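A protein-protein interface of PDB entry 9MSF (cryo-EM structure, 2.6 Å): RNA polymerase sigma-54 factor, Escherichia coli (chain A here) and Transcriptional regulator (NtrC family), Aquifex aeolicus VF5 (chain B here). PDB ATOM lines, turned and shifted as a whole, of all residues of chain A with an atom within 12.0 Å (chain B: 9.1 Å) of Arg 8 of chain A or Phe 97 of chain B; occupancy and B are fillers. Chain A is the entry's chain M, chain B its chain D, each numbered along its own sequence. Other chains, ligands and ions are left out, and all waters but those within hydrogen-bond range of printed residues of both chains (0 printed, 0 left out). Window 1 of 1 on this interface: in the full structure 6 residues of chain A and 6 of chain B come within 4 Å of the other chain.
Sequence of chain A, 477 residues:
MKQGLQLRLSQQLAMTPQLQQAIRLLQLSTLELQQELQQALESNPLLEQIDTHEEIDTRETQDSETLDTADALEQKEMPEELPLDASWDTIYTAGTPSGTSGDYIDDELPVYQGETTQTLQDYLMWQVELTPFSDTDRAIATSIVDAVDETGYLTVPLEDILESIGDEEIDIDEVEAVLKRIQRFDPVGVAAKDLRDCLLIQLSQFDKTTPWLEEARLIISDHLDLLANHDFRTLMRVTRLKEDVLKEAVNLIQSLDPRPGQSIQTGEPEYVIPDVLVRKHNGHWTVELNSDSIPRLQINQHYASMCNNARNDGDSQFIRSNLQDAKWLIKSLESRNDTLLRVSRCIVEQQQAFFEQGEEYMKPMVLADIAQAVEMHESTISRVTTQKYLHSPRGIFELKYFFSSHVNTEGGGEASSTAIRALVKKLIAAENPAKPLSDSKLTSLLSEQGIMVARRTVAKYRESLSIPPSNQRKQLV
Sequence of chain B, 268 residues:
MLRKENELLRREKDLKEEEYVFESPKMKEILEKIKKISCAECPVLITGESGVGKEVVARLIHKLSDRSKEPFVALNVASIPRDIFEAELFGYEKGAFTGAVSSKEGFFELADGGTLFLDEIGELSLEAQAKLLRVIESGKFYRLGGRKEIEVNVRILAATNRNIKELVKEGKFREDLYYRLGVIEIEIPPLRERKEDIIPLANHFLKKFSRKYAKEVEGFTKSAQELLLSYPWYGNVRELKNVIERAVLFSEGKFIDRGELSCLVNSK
OG1 of Thr 98 of chain B sits at hydrogen-bond distance from N of Ser 10 of chain A, 3.0 Å away. The backbone carbonyl oxygen (O) of Arg 8 of chain A is in hydrogen-bond range of the backbone NH (N) of Thr 98 of chain B (3.0 Å).
Leu 5 of chain A touches Asp 83 of chain B (O to CB, 3.2 Å). CG of Gln 6 of chain A touches OD2 of Asp 83 of chain B, at 3.9 Å. CD2 of Leu 7 of chain A touches CG2 of Ile 84 of chain B, 3.7 Å away. CB of Ala 87 of chain B touches CD1 of Leu 7 of chain A (3.8 Å). Phe 97 of chain B touches Leu 7 of chain A. Phe 97 of chain B touches Arg 8 of chain A (CB to O, 3.7 Å). Leu 9 of chain A touches Ala 96 of chain B. Leu 9 of chain A touches Phe 97 of chain B (CD2 to CA, 3.8 Å). Thr 98 of chain B touches Leu 9 of chain A (OG1 to CA, 3.6 Å).
Printed residues of chain B within 4 Å of Leu 5 of chain A: Asp 83. Arg 8 of chain A touches just these residues of chain B: Phe 97 and Thr 98. Printed residues of chain B within 4 Å of Leu 9 of chain A: Ala 96 (3.8 Å), Phe 97 (3.8 Å) and Thr 98 (3.6 Å). Of the printed residues of chain B, Ser 10 of chain A touches Thr 98. No residue of chain A comes within 4 Å of Gly 95 of chain B. Ala 96 of chain B touches one residue of chain A. No residue of chain A comes within 4 Å of Gly 99 of chain B. No residue of chain A comes within 4 Å of Ala 100 of chain B. No residue of chain A comes within 4 Å of Leu 144 of chain B. The nearest residue of chain B that does not touch Arg 8 of chain A is Gly 99 of chain B (5.8 Å). The nearest residue of chain A that does not touch Phe 97 of chain B is Gln 6 of chain A (5.6 Å). The nearest printed residue of chain B that does not touch Leu 5 of chain A is Ile 84 of chain B (4.2 Å).
Of the 21 printed residues of chain B, 6 touch a printed residue of chain A. Hydrophobic or aromatic side chains of chain B within 4 Å of the printed part of chain A: Ile 84, Ala 87 and Phe 97. Among the printed residues, no Asp or Glu carboxylate lies within 4 Å of a Lys or Arg side-chain nitrogen of the other chain.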
ATOM      1  N   LYS A   2      20.205   7.363 -33.663  1.00  0.00           N
ATOM      2  CA  LYS A   2      19.588   6.127 -33.198  1.00  0.00           C
ATOM      3  C   LYS A   2      19.374   6.155 -31.690  1.00  0.00           C
ATOM      4  O   LYS A   2      19.489   7.204 -31.056  1.00  0.00           O
ATOM      5  CB  LYS A   2      20.447   4.921 -33.585  1.00  0.00           C
ATOM      6  N   GLN A   3      19.062   4.994 -31.118  1.00  0.00           N
ATOM      7  CA  GLN A   3      18.870   4.878 -29.678  1.00  0.00           C
ATOM      8  C   GLN A   3      20.228   4.849 -28.989  1.00  0.00           C
ATOM      9  O   GLN A   3      21.029   3.936 -29.219  1.00  0.00           O
ATOM     10  CB  GLN A   3      18.068   3.624 -29.339  1.00  0.00           C
ATOM     11  CG  GLN A   3      16.611   3.668 -29.775  1.00  0.00           C
ATOM     12  CD  GLN A   3      16.432   3.397 -31.255  1.00  0.00           C
ATOM     13  OE1 GLN A   3      15.731   4.131 -31.951  1.00  0.00           O
ATOM     14  NE2 GLN A   3      17.061   2.336 -31.742  1.00  0.00           N
ATOM     15  N   GLY A   4      20.488   5.844 -28.150  1.00  0.00           N
ATOM     16  CA  GLY A   4      21.752   5.914 -27.445  1.00  0.00           C
ATOM     17  C   GLY A   4      21.694   6.939 -26.338  1.00  0.00           C
ATOM     18  O   GLY A   4      20.800   7.790 -26.296  1.00  0.00           O
ATOM     19  N   LEU A   5      22.664   6.841 -25.434  1.00  0.00           N
ATOM     20  CA  LEU A   5      22.796   7.755 -24.306  1.00  0.00           C
ATOM     21  C   LEU A   5      24.081   8.551 -24.485  1.00  0.00           C
ATOM     22  O   LEU A   5      25.176   7.984 -24.433  1.00  0.00           O
ATOM     23  CB  LEU A   5      22.813   6.987 -22.985  1.00  0.00           C
ATOM     24  CG  LEU A   5      21.783   5.862 -22.864  1.00  0.00           C
ATOM     25  CD1 LEU A   5      21.961   5.111 -21.559  1.00  0.00           C
ATOM     26  CD2 LEU A   5      20.371   6.407 -22.982  1.00  0.00           C
ATOM     27  N   GLN A   6      23.947   9.859 -24.696  1.00  0.00           N
ATOM     28  CA  GLN A   6      25.087  10.704 -25.015  1.00  0.00           C
ATOM     29  C   GLN A   6      24.963  12.040 -24.296  1.00  0.00           C
ATOM     30  O   GLN A   6      23.877  12.453 -23.885  1.00  0.00           O
ATOM     31  CB  GLN A   6      25.210  10.943 -26.526  1.00  0.00           C
ATOM     32  CG  GLN A   6      25.280   9.678 -27.364  1.00  0.00           C
ATOM     33  CD  GLN A   6      25.248   9.962 -28.850  1.00  0.00           C
ATOM     34  OE1 GLN A   6      25.793  10.963 -29.314  1.00  0.00           O
ATOM     35  NE2 GLN A   6      24.600   9.084 -29.606  1.00  0.00           N
ATOM     36  N   LEU A   7      26.103  12.708 -24.148  1.00  0.00           N
ATOM     37  CA  LEU A   7      26.173  14.076 -23.657  1.00  0.00           C
ATOM     38  C   LEU A   7      26.530  14.981 -24.826  1.00  0.00           C
ATOM     39  O   LEU A   7      27.546  14.760 -25.492  1.00  0.00           O
ATOM     40  CB  LEU A   7      27.218  14.210 -22.546  1.00  0.00           C
ATOM     41  CG  LEU A   7      27.244  13.133 -21.464  1.00  0.00           C
ATOM     42  CD1 LEU A   7      28.406  13.370 -20.516  1.00  0.00           C
ATOM     43  CD2 LEU A   7      25.932  13.097 -20.705  1.00  0.00           C
ATOM     44  N   ARG A   8      25.705  15.995 -25.075  1.00  0.00           N
ATOM     45  CA  ARG A   8      25.859  16.799 -26.278  1.00  0.00           C
ATOM     46  C   ARG A   8      25.300  18.194 -26.048  1.00  0.00           C
ATOM     47  O   ARG A   8      24.573  18.450 -25.084  1.00  0.00           O
ATOM     48  CB  ARG A   8      25.170  16.136 -27.473  1.00  0.00           C
ATOM     49  CG  ARG A   8      23.763  15.652 -27.173  1.00  0.00           C
ATOM     50  CD  ARG A   8      23.082  15.071 -28.402  1.00  0.00           C
ATOM     51  NE  ARG A   8      23.808  13.937 -28.961  1.00  0.00           N
ATOM     52  CZ  ARG A   8      24.574  13.998 -30.042  1.00  0.00           C
ATOM     53  NH1 ARG A   8      24.740  15.128 -30.708  1.00  0.00           N
ATOM     54  NH2 ARG A   8      25.185  12.896 -30.467  1.00  0.00           N
ATOM     55  N   LEU A   9      25.659  19.102 -26.953  1.00  0.00           N
ATOM     56  CA  LEU A   9      25.167  20.474 -26.961  1.00  0.00           C
ATOM     57  C   LEU A   9      24.178  20.600 -28.114  1.00  0.00           C
ATOM     58  O   LEU A   9      24.556  20.450 -29.280  1.00  0.00           O
ATOM     59  CB  LEU A   9      26.318  21.467 -27.116  1.00  0.00           C
ATOM     60  CG  LEU A   9      27.566  21.239 -26.262  1.00  0.00           C
ATOM     61  CD1 LEU A   9      28.655  22.222 -26.649  1.00  0.00           C
ATOM     62  CD2 LEU A   9      27.242  21.357 -24.788  1.00  0.00           C
ATOM     63  N   SER A  10      22.916  20.873 -27.792  1.00  0.00           N
ATOM     64  CA  SER A  10      21.852  20.903 -28.784  1.00  0.00           C
ATOM     65  C   SER A  10      20.959  22.116 -28.563  1.00  0.00           C
ATOM     66  O   SER A  10      21.024  22.789 -27.531  1.00  0.00           O
ATOM     67  CB  SER A  10      21.013  19.619 -28.742  1.00  0.00           C
ATOM     68  OG  SER A  10      21.805  18.479 -29.020  1.00  0.00           O
ATOM     69  N   GLN A  11      20.119  22.388 -29.558  1.00  0.00           N
ATOM     70  CA  GLN A  11      19.103  23.428 -29.488  1.00  0.00           C
ATOM     71  C   GLN A  11      17.741  22.767 -29.629  1.00  0.00           C
ATOM     72  O   GLN A  11      17.429  22.206 -30.684  1.00  0.00           O
ATOM     73  CB  GLN A  11      19.313  24.477 -30.580  1.00  0.00           C
ATOM     74  CG  GLN A  11      20.644  25.192 -30.493  1.00  0.00           C
ATOM     75  CD  GLN A  11      20.859  26.149 -31.641  1.00  0.00           C
ATOM     76  OE1 GLN A  11      21.662  27.075 -31.550  1.00  0.00           O
ATOM     77  NE2 GLN A  11      20.141  25.930 -32.735  1.00  0.00           N
ATOM     78  N   GLN A  12      16.934  22.834 -28.573  1.00  0.00           N
ATOM     79  CA  GLN A  12      15.685  22.095 -28.504  1.00  0.00           C
ATOM     80  C   GLN A  12      14.564  22.990 -27.995  1.00  0.00           C
ATOM     81  O   GLN A  12      14.798  24.024 -27.367  1.00  0.00           O
ATOM     82  CB  GLN A  12      15.812  20.867 -27.591  1.00  0.00           C
ATOM     83  CG  GLN A  12      16.798  19.822 -28.077  1.00  0.00           C
ATOM     84  CD  GLN A  12      16.991  18.699 -27.080  1.00  0.00           C
ATOM     85  OE1 GLN A  12      16.641  18.831 -25.906  1.00  0.00           O
ATOM     86  NE2 GLN A  12      17.546  17.585 -27.540  1.00  0.00           N
ATOM     87  N   ALA A  14      11.679  22.844 -25.404  1.00  0.00           N
ATOM     88  CA  ALA A  14      11.322  22.074 -24.223  1.00  0.00           C
ATOM     89  C   ALA A  14       9.937  22.460 -23.718  1.00  0.00           C
ATOM     90  O   ALA A  14       9.519  23.617 -23.814  1.00  0.00           O
ATOM     91  CB  ALA A  14      12.357  22.271 -23.113  1.00  0.00           C
ATOM     92  N   ASP B  83      29.553   6.563 -23.634  1.00  0.00           N
ATOM     93  CA  ASP B  83      29.503   8.003 -23.853  1.00  0.00           C
ATOM     94  C   ASP B  83      29.330   8.812 -22.575  1.00  0.00           C
ATOM     95  O   ASP B  83      29.499  10.035 -22.615  1.00  0.00           O
ATOM     96  CB  ASP B  83      28.373   8.347 -24.827  1.00  0.00           C
ATOM     97  CG  ASP B  83      28.604   7.776 -26.212  1.00  0.00           C
ATOM     98  OD1 ASP B  83      28.395   6.560 -26.399  1.00  0.00           O
ATOM     99  OD2 ASP B  83      28.997   8.545 -27.114  1.00  0.00           O
ATOM    100  N   ILE B  84      29.001   8.178 -21.452  1.00  0.00           N
ATOM    101  CA  ILE B  84      28.837   8.885 -20.190  1.00  0.00           C
ATOM    102  C   ILE B  84      29.823   8.384 -19.137  1.00  0.00           C
ATOM    103  O   ILE B  84      29.587   8.534 -17.945  1.00  0.00           O
ATOM    104  CB  ILE B  84      27.383   8.796 -19.686  1.00  0.00           C
ATOM    105  CG1 ILE B  84      26.995   7.345 -19.406  1.00  0.00           C
ATOM    106  CG2 ILE B  84      26.430   9.409 -20.699  1.00  0.00           C
ATOM    107  CD1 ILE B  84      25.596   7.192 -18.853  1.00  0.00           C
ATOM    108  N   GLU B  86      32.904   9.484 -18.416  1.00  0.00           N
ATOM    109  CA  GLU B  86      33.531  10.578 -17.681  1.00  0.00           C
ATOM    110  C   GLU B  86      32.562  11.211 -16.690  1.00  0.00           C
ATOM    111  O   GLU B  86      32.954  11.562 -15.572  1.00  0.00           O
ATOM    112  CB  GLU B  86      34.064  11.633 -18.649  1.00  0.00           C
ATOM    113  CG  GLU B  86      35.012  11.103 -19.715  1.00  0.00           C
ATOM    114  CD  GLU B  86      34.284  10.589 -20.943  1.00  0.00           C
ATOM    115  OE1 GLU B  86      33.035  10.576 -20.936  1.00  0.00           O
ATOM    116  OE2 GLU B  86      34.961  10.201 -21.918  1.00  0.00           O
ATOM    117  N   ALA B  87      31.299  11.376 -17.084  1.00  0.00           N
ATOM    118  CA  ALA B  87      30.314  11.963 -16.180  1.00  0.00           C
ATOM    119  C   ALA B  87      30.075  11.071 -14.968  1.00  0.00           C
ATOM    120  O   ALA B  87      29.950  11.567 -13.841  1.00  0.00           O
ATOM    121  CB  ALA B  87      29.005  12.222 -16.923  1.00  0.00           C
ATOM    122  N   GLU B  88      29.997   9.756 -15.179  1.00  0.00           N
ATOM    123  CA  GLU B  88      29.825   8.836 -14.059  1.00  0.00           C
ATOM    124  C   GLU B  88      31.037   8.849 -13.136  1.00  0.00           C
ATOM    125  O   GLU B  88      30.888   8.859 -11.910  1.00  0.00           O
ATOM    126  CB  GLU B  88      29.569   7.420 -14.578  1.00  0.00           C
ATOM    127  CG  GLU B  88      28.285   7.263 -15.375  1.00  0.00           C
ATOM    128  CD  GLU B  88      27.068   7.072 -14.494  1.00  0.00           C
ATOM    129  OE1 GLU B  88      27.170   6.340 -13.488  1.00  0.00           O
ATOM    130  OE2 GLU B  88      26.009   7.655 -14.808  1.00  0.00           O
ATOM    131  N   GLY B  91      31.820  13.235 -12.418  1.00  0.00           N
ATOM    132  CA  GLY B  91      30.754  14.183 -12.174  1.00  0.00           C
ATOM    133  C   GLY B  91      30.812  15.352 -13.137  1.00  0.00           C
ATOM    134  O   GLY B  91      31.707  15.476 -13.974  1.00  0.00           O
ATOM    135  N   TYR B  92      29.826  16.235 -13.010  1.00  0.00           N
ATOM    136  CA  TYR B  92      29.737  17.383 -13.898  1.00  0.00           C
ATOM    137  C   TYR B  92      29.220  18.587 -13.127  1.00  0.00           C
ATOM    138  O   TYR B  92      28.673  18.463 -12.029  1.00  0.00           O
ATOM    139  CB  TYR B  92      28.840  17.092 -15.108  1.00  0.00           C
ATOM    140  CG  TYR B  92      27.411  16.743 -14.760  1.00  0.00           C
ATOM    141  CD1 TYR B  92      26.441  17.728 -14.653  1.00  0.00           C
ATOM    142  CD2 TYR B  92      27.030  15.425 -14.551  1.00  0.00           C
ATOM    143  CE1 TYR B  92      25.139  17.416 -14.341  1.00  0.00           C
ATOM    144  CE2 TYR B  92      25.727  15.103 -14.237  1.00  0.00           C
ATOM    145  CZ  TYR B  92      24.786  16.103 -14.133  1.00  0.00           C
ATOM    146  OH  TYR B  92      23.484  15.793 -13.821  1.00  0.00           O
ATOM    147  N   GLU B  93      29.410  19.759 -13.719  1.00  0.00           N
ATOM    148  CA  GLU B  93      28.917  21.014 -13.176  1.00  0.00           C
ATOM    149  C   GLU B  93      27.653  21.435 -13.918  1.00  0.00           C
ATOM    150  O   GLU B  93      27.304  20.889 -14.966  1.00  0.00           O
ATOM    151  CB  GLU B  93      29.989  22.102 -13.282  1.00  0.00           C
ATOM    152  CG  GLU B  93      30.004  23.082 -12.123  1.00  0.00           C
ATOM    153  CD  GLU B  93      30.803  22.571 -10.943  1.00  0.00           C
ATOM    154  OE1 GLU B  93      31.743  21.779 -11.161  1.00  0.00           O
ATOM    155  OE2 GLU B  93      30.493  22.957  -9.796  1.00  0.00           O
ATOM    156  N   LYS B  94      26.959  22.419 -13.355  1.00  0.00           N
ATOM    157  CA  LYS B  94      25.729  22.904 -13.968  1.00  0.00           C
ATOM    158  C   LYS B  94      26.034  23.592 -15.292  1.00  0.00           C
ATOM    159  O   LYS B  94      26.965  24.396 -15.388  1.00  0.00           O
ATOM    160  CB  LYS B  94      25.009  23.864 -13.024  1.00  0.00           C
ATOM    161  CG  LYS B  94      23.687  24.383 -13.563  1.00  0.00           C
ATOM    162  CD  LYS B  94      22.939  25.183 -12.511  1.00  0.00           C
ATOM    163  CE  LYS B  94      23.751  26.378 -12.041  1.00  0.00           C
ATOM    164  NZ  LYS B  94      23.031  27.156 -10.995  1.00  0.00           N
ATOM    165  N   GLY B  95      25.245  23.276 -16.315  1.00  0.00           N
ATOM    166  CA  GLY B  95      25.442  23.855 -17.628  1.00  0.00           C
ATOM    167  C   GLY B  95      26.536  23.222 -18.456  1.00  0.00           C
ATOM    168  O   GLY B  95      26.912  23.790 -19.486  1.00  0.00           O
ATOM    169  N   ALA B  96      27.064  22.070 -18.037  1.00  0.00           N
ATOM    170  CA  ALA B  96      28.138  21.429 -18.791  1.00  0.00           C
ATOM    171  C   ALA B  96      27.665  20.993 -20.171  1.00  0.00           C
ATOM    172  O   ALA B  96      28.390  21.145 -21.160  1.00  0.00           O
ATOM    173  CB  ALA B  96      28.686  20.235 -18.011  1.00  0.00           C
ATOM    174  N   PHE B  97      26.453  20.450 -20.258  1.00  0.00           N
ATOM    175  CA  PHE B  97      25.875  20.013 -21.520  1.00  0.00           C
ATOM    176  C   PHE B  97      24.376  20.270 -21.481  1.00  0.00           C
ATOM    177  O   PHE B  97      23.844  20.826 -20.517  1.00  0.00           O
ATOM    178  CB  PHE B  97      26.188  18.536 -21.792  1.00  0.00           C
ATOM    179  CG  PHE B  97      25.809  17.613 -20.665  1.00  0.00           C
ATOM    180  CD1 PHE B  97      26.707  17.339 -19.647  1.00  0.00           C
ATOM    181  CD2 PHE B  97      24.561  17.017 -20.627  1.00  0.00           C
ATOM    182  CE1 PHE B  97      26.361  16.492 -18.611  1.00  0.00           C
ATOM    183  CE2 PHE B  97      24.213  16.170 -19.592  1.00  0.00           C
ATOM    184  CZ  PHE B  97      25.113  15.907 -18.585  1.00  0.00           C
ATOM    185  N   THR B  98      23.686  19.862 -22.543  1.00  0.00           N
ATOM    186  CA  THR B  98      22.240  20.027 -22.620  1.00  0.00           C
ATOM    187  C   THR B  98      21.570  18.953 -21.773  1.00  0.00           C
ATOM    188  O   THR B  98      21.711  17.757 -22.051  1.00  0.00           O
ATOM    189  CB  THR B  98      21.763  19.947 -24.067  1.00  0.00           C
ATOM    190  OG1 THR B  98      22.325  21.029 -24.820  1.00  0.00           O
ATOM    191  CG2 THR B  98      20.248  20.028 -24.132  1.00  0.00           C
ATOM    192  N   GLY B  99      20.842  19.378 -20.744  1.00  0.00           N
ATOM    193  CA  GLY B  99      20.223  18.474 -19.797  1.00  0.00           C
ATOM    194  C   GLY B  99      20.869  18.464 -18.429  1.00  0.00           C
ATOM    195  O   GLY B  99      20.324  17.837 -17.512  1.00  0.00           O
ATOM    196  N   ALA B 100      22.009  19.131 -18.261  1.00  0.00           N
ATOM    197  CA  ALA B 100      22.674  19.238 -16.964  1.00  0.00           C
ATOM    198  C   ALA B 100      22.022  20.376 -16.194  1.00  0.00           C
ATOM    199  O   ALA B 100      22.350  21.550 -16.372  1.00  0.00           O
ATOM    200  CB  ALA B 100      24.169  19.464 -17.143  1.00  0.00           C
ATOM    201  N   VAL B 101      21.079  20.023 -15.319  1.00  0.00           N
ATOM    202  CA  VAL B 101      20.317  21.031 -14.590  1.00  0.00           C
ATOM    203  C   VAL B 101      20.902  21.352 -13.219  1.00  0.00           C
ATOM    204  O   VAL B 101      20.581  22.405 -12.652  1.00  0.00           O
ATOM    205  CB  VAL B 101      18.850  20.593 -14.435  1.00  0.00           C
ATOM    206  CG1 VAL B 101      18.152  20.598 -15.786  1.00  0.00           C
ATOM    207  CG2 VAL B 101      18.775  19.216 -13.800  1.00  0.00           C
ATOM    208  N   SER B 102      21.746  20.481 -12.671  1.00  0.00           N
ATOM    209  CA  SER B 102      22.359  20.730 -11.375  1.00  0.00           C
ATOM    210  C   SER B 102      23.675  19.974 -11.292  1.00  0.00           C
ATOM    211  O   SER B 102      23.880  18.969 -11.977  1.00  0.00           O
ATOM    212  CB  SER B 102      21.430  20.321 -10.226  1.00  0.00           C
ATOM    213  OG  SER B 102      22.029  20.581  -8.969  1.00  0.00           O
ATOM    214  N   SER B 103      24.568  20.470 -10.442  1.00  0.00           N
ATOM    215  CA  SER B 103      25.866  19.838 -10.271  1.00  0.00           C
ATOM    216  C   SER B 103      25.720  18.488  -9.578  1.00  0.00           C
ATOM    217  O   SER B 103      24.844  18.287  -8.733  1.00  0.00           O
ATOM    218  CB  SER B 103      26.799  20.741  -9.466  1.00  0.00           C
ATOM    219  OG  SER B 103      26.294  20.966  -8.162  1.00  0.00           O
ATOM    220  N   LYS B 104      26.594  17.555  -9.947  1.00  0.00           N
ATOM    221  CA  LYS B 104      26.554  16.205  -9.407  1.00  0.00           C
ATOM    222  C   LYS B 104      27.970  15.657  -9.327  1.00  0.00           C
ATOM    223  O   LYS B 104      28.773  15.863 -10.240  1.00  0.00           O
ATOM    224  CB  LYS B 104      25.669  15.296 -10.267  1.00  0.00           C
ATOM    225  CG  LYS B 104      25.896  13.810 -10.057  1.00  0.00           C
ATOM    226  CD  LYS B 104      24.779  12.990 -10.672  1.00  0.00           C
ATOM    227  CE  LYS B 104      23.498  13.143  -9.875  1.00  0.00           C
ATOM    228  NZ  LYS B 104      23.679  12.694  -8.467  1.00  0.00           N
ATOM    229  N   LEU B 144      33.366  17.704 -15.163  1.00  0.00           N
ATOM    230  CA  LEU B 144      32.922  18.108 -16.493  1.00  0.00           C
ATOM    231  C   LEU B 144      32.272  19.483 -16.410  1.00  0.00           C
ATOM    232  O   LEU B 144      31.159  19.622 -15.897  1.00  0.00           O
ATOM    233  CB  LEU B 144      31.955  17.078 -17.068  1.00  0.00           C
ATOM    234  CG  LEU B 144      32.547  16.055 -18.037  1.00  0.00           C
ATOM    235  CD1 LEU B 144      33.636  15.235 -17.368  1.00  0.00           C
ATOM    236  CD2 LEU B 144      31.458  15.155 -18.594  1.00  0.00           C
ATOM    237  N   GLY B 145      32.962  20.500 -16.916  1.00  0.00           N
ATOM    238  CA  GLY B 145      32.499  21.864 -16.816  1.00  0.00           C
ATOM    239  C   GLY B 145      33.010  22.627 -15.614  1.00  0.00           C
ATOM    240  O   GLY B 145      32.629  23.789 -15.433  1.00  0.00           O
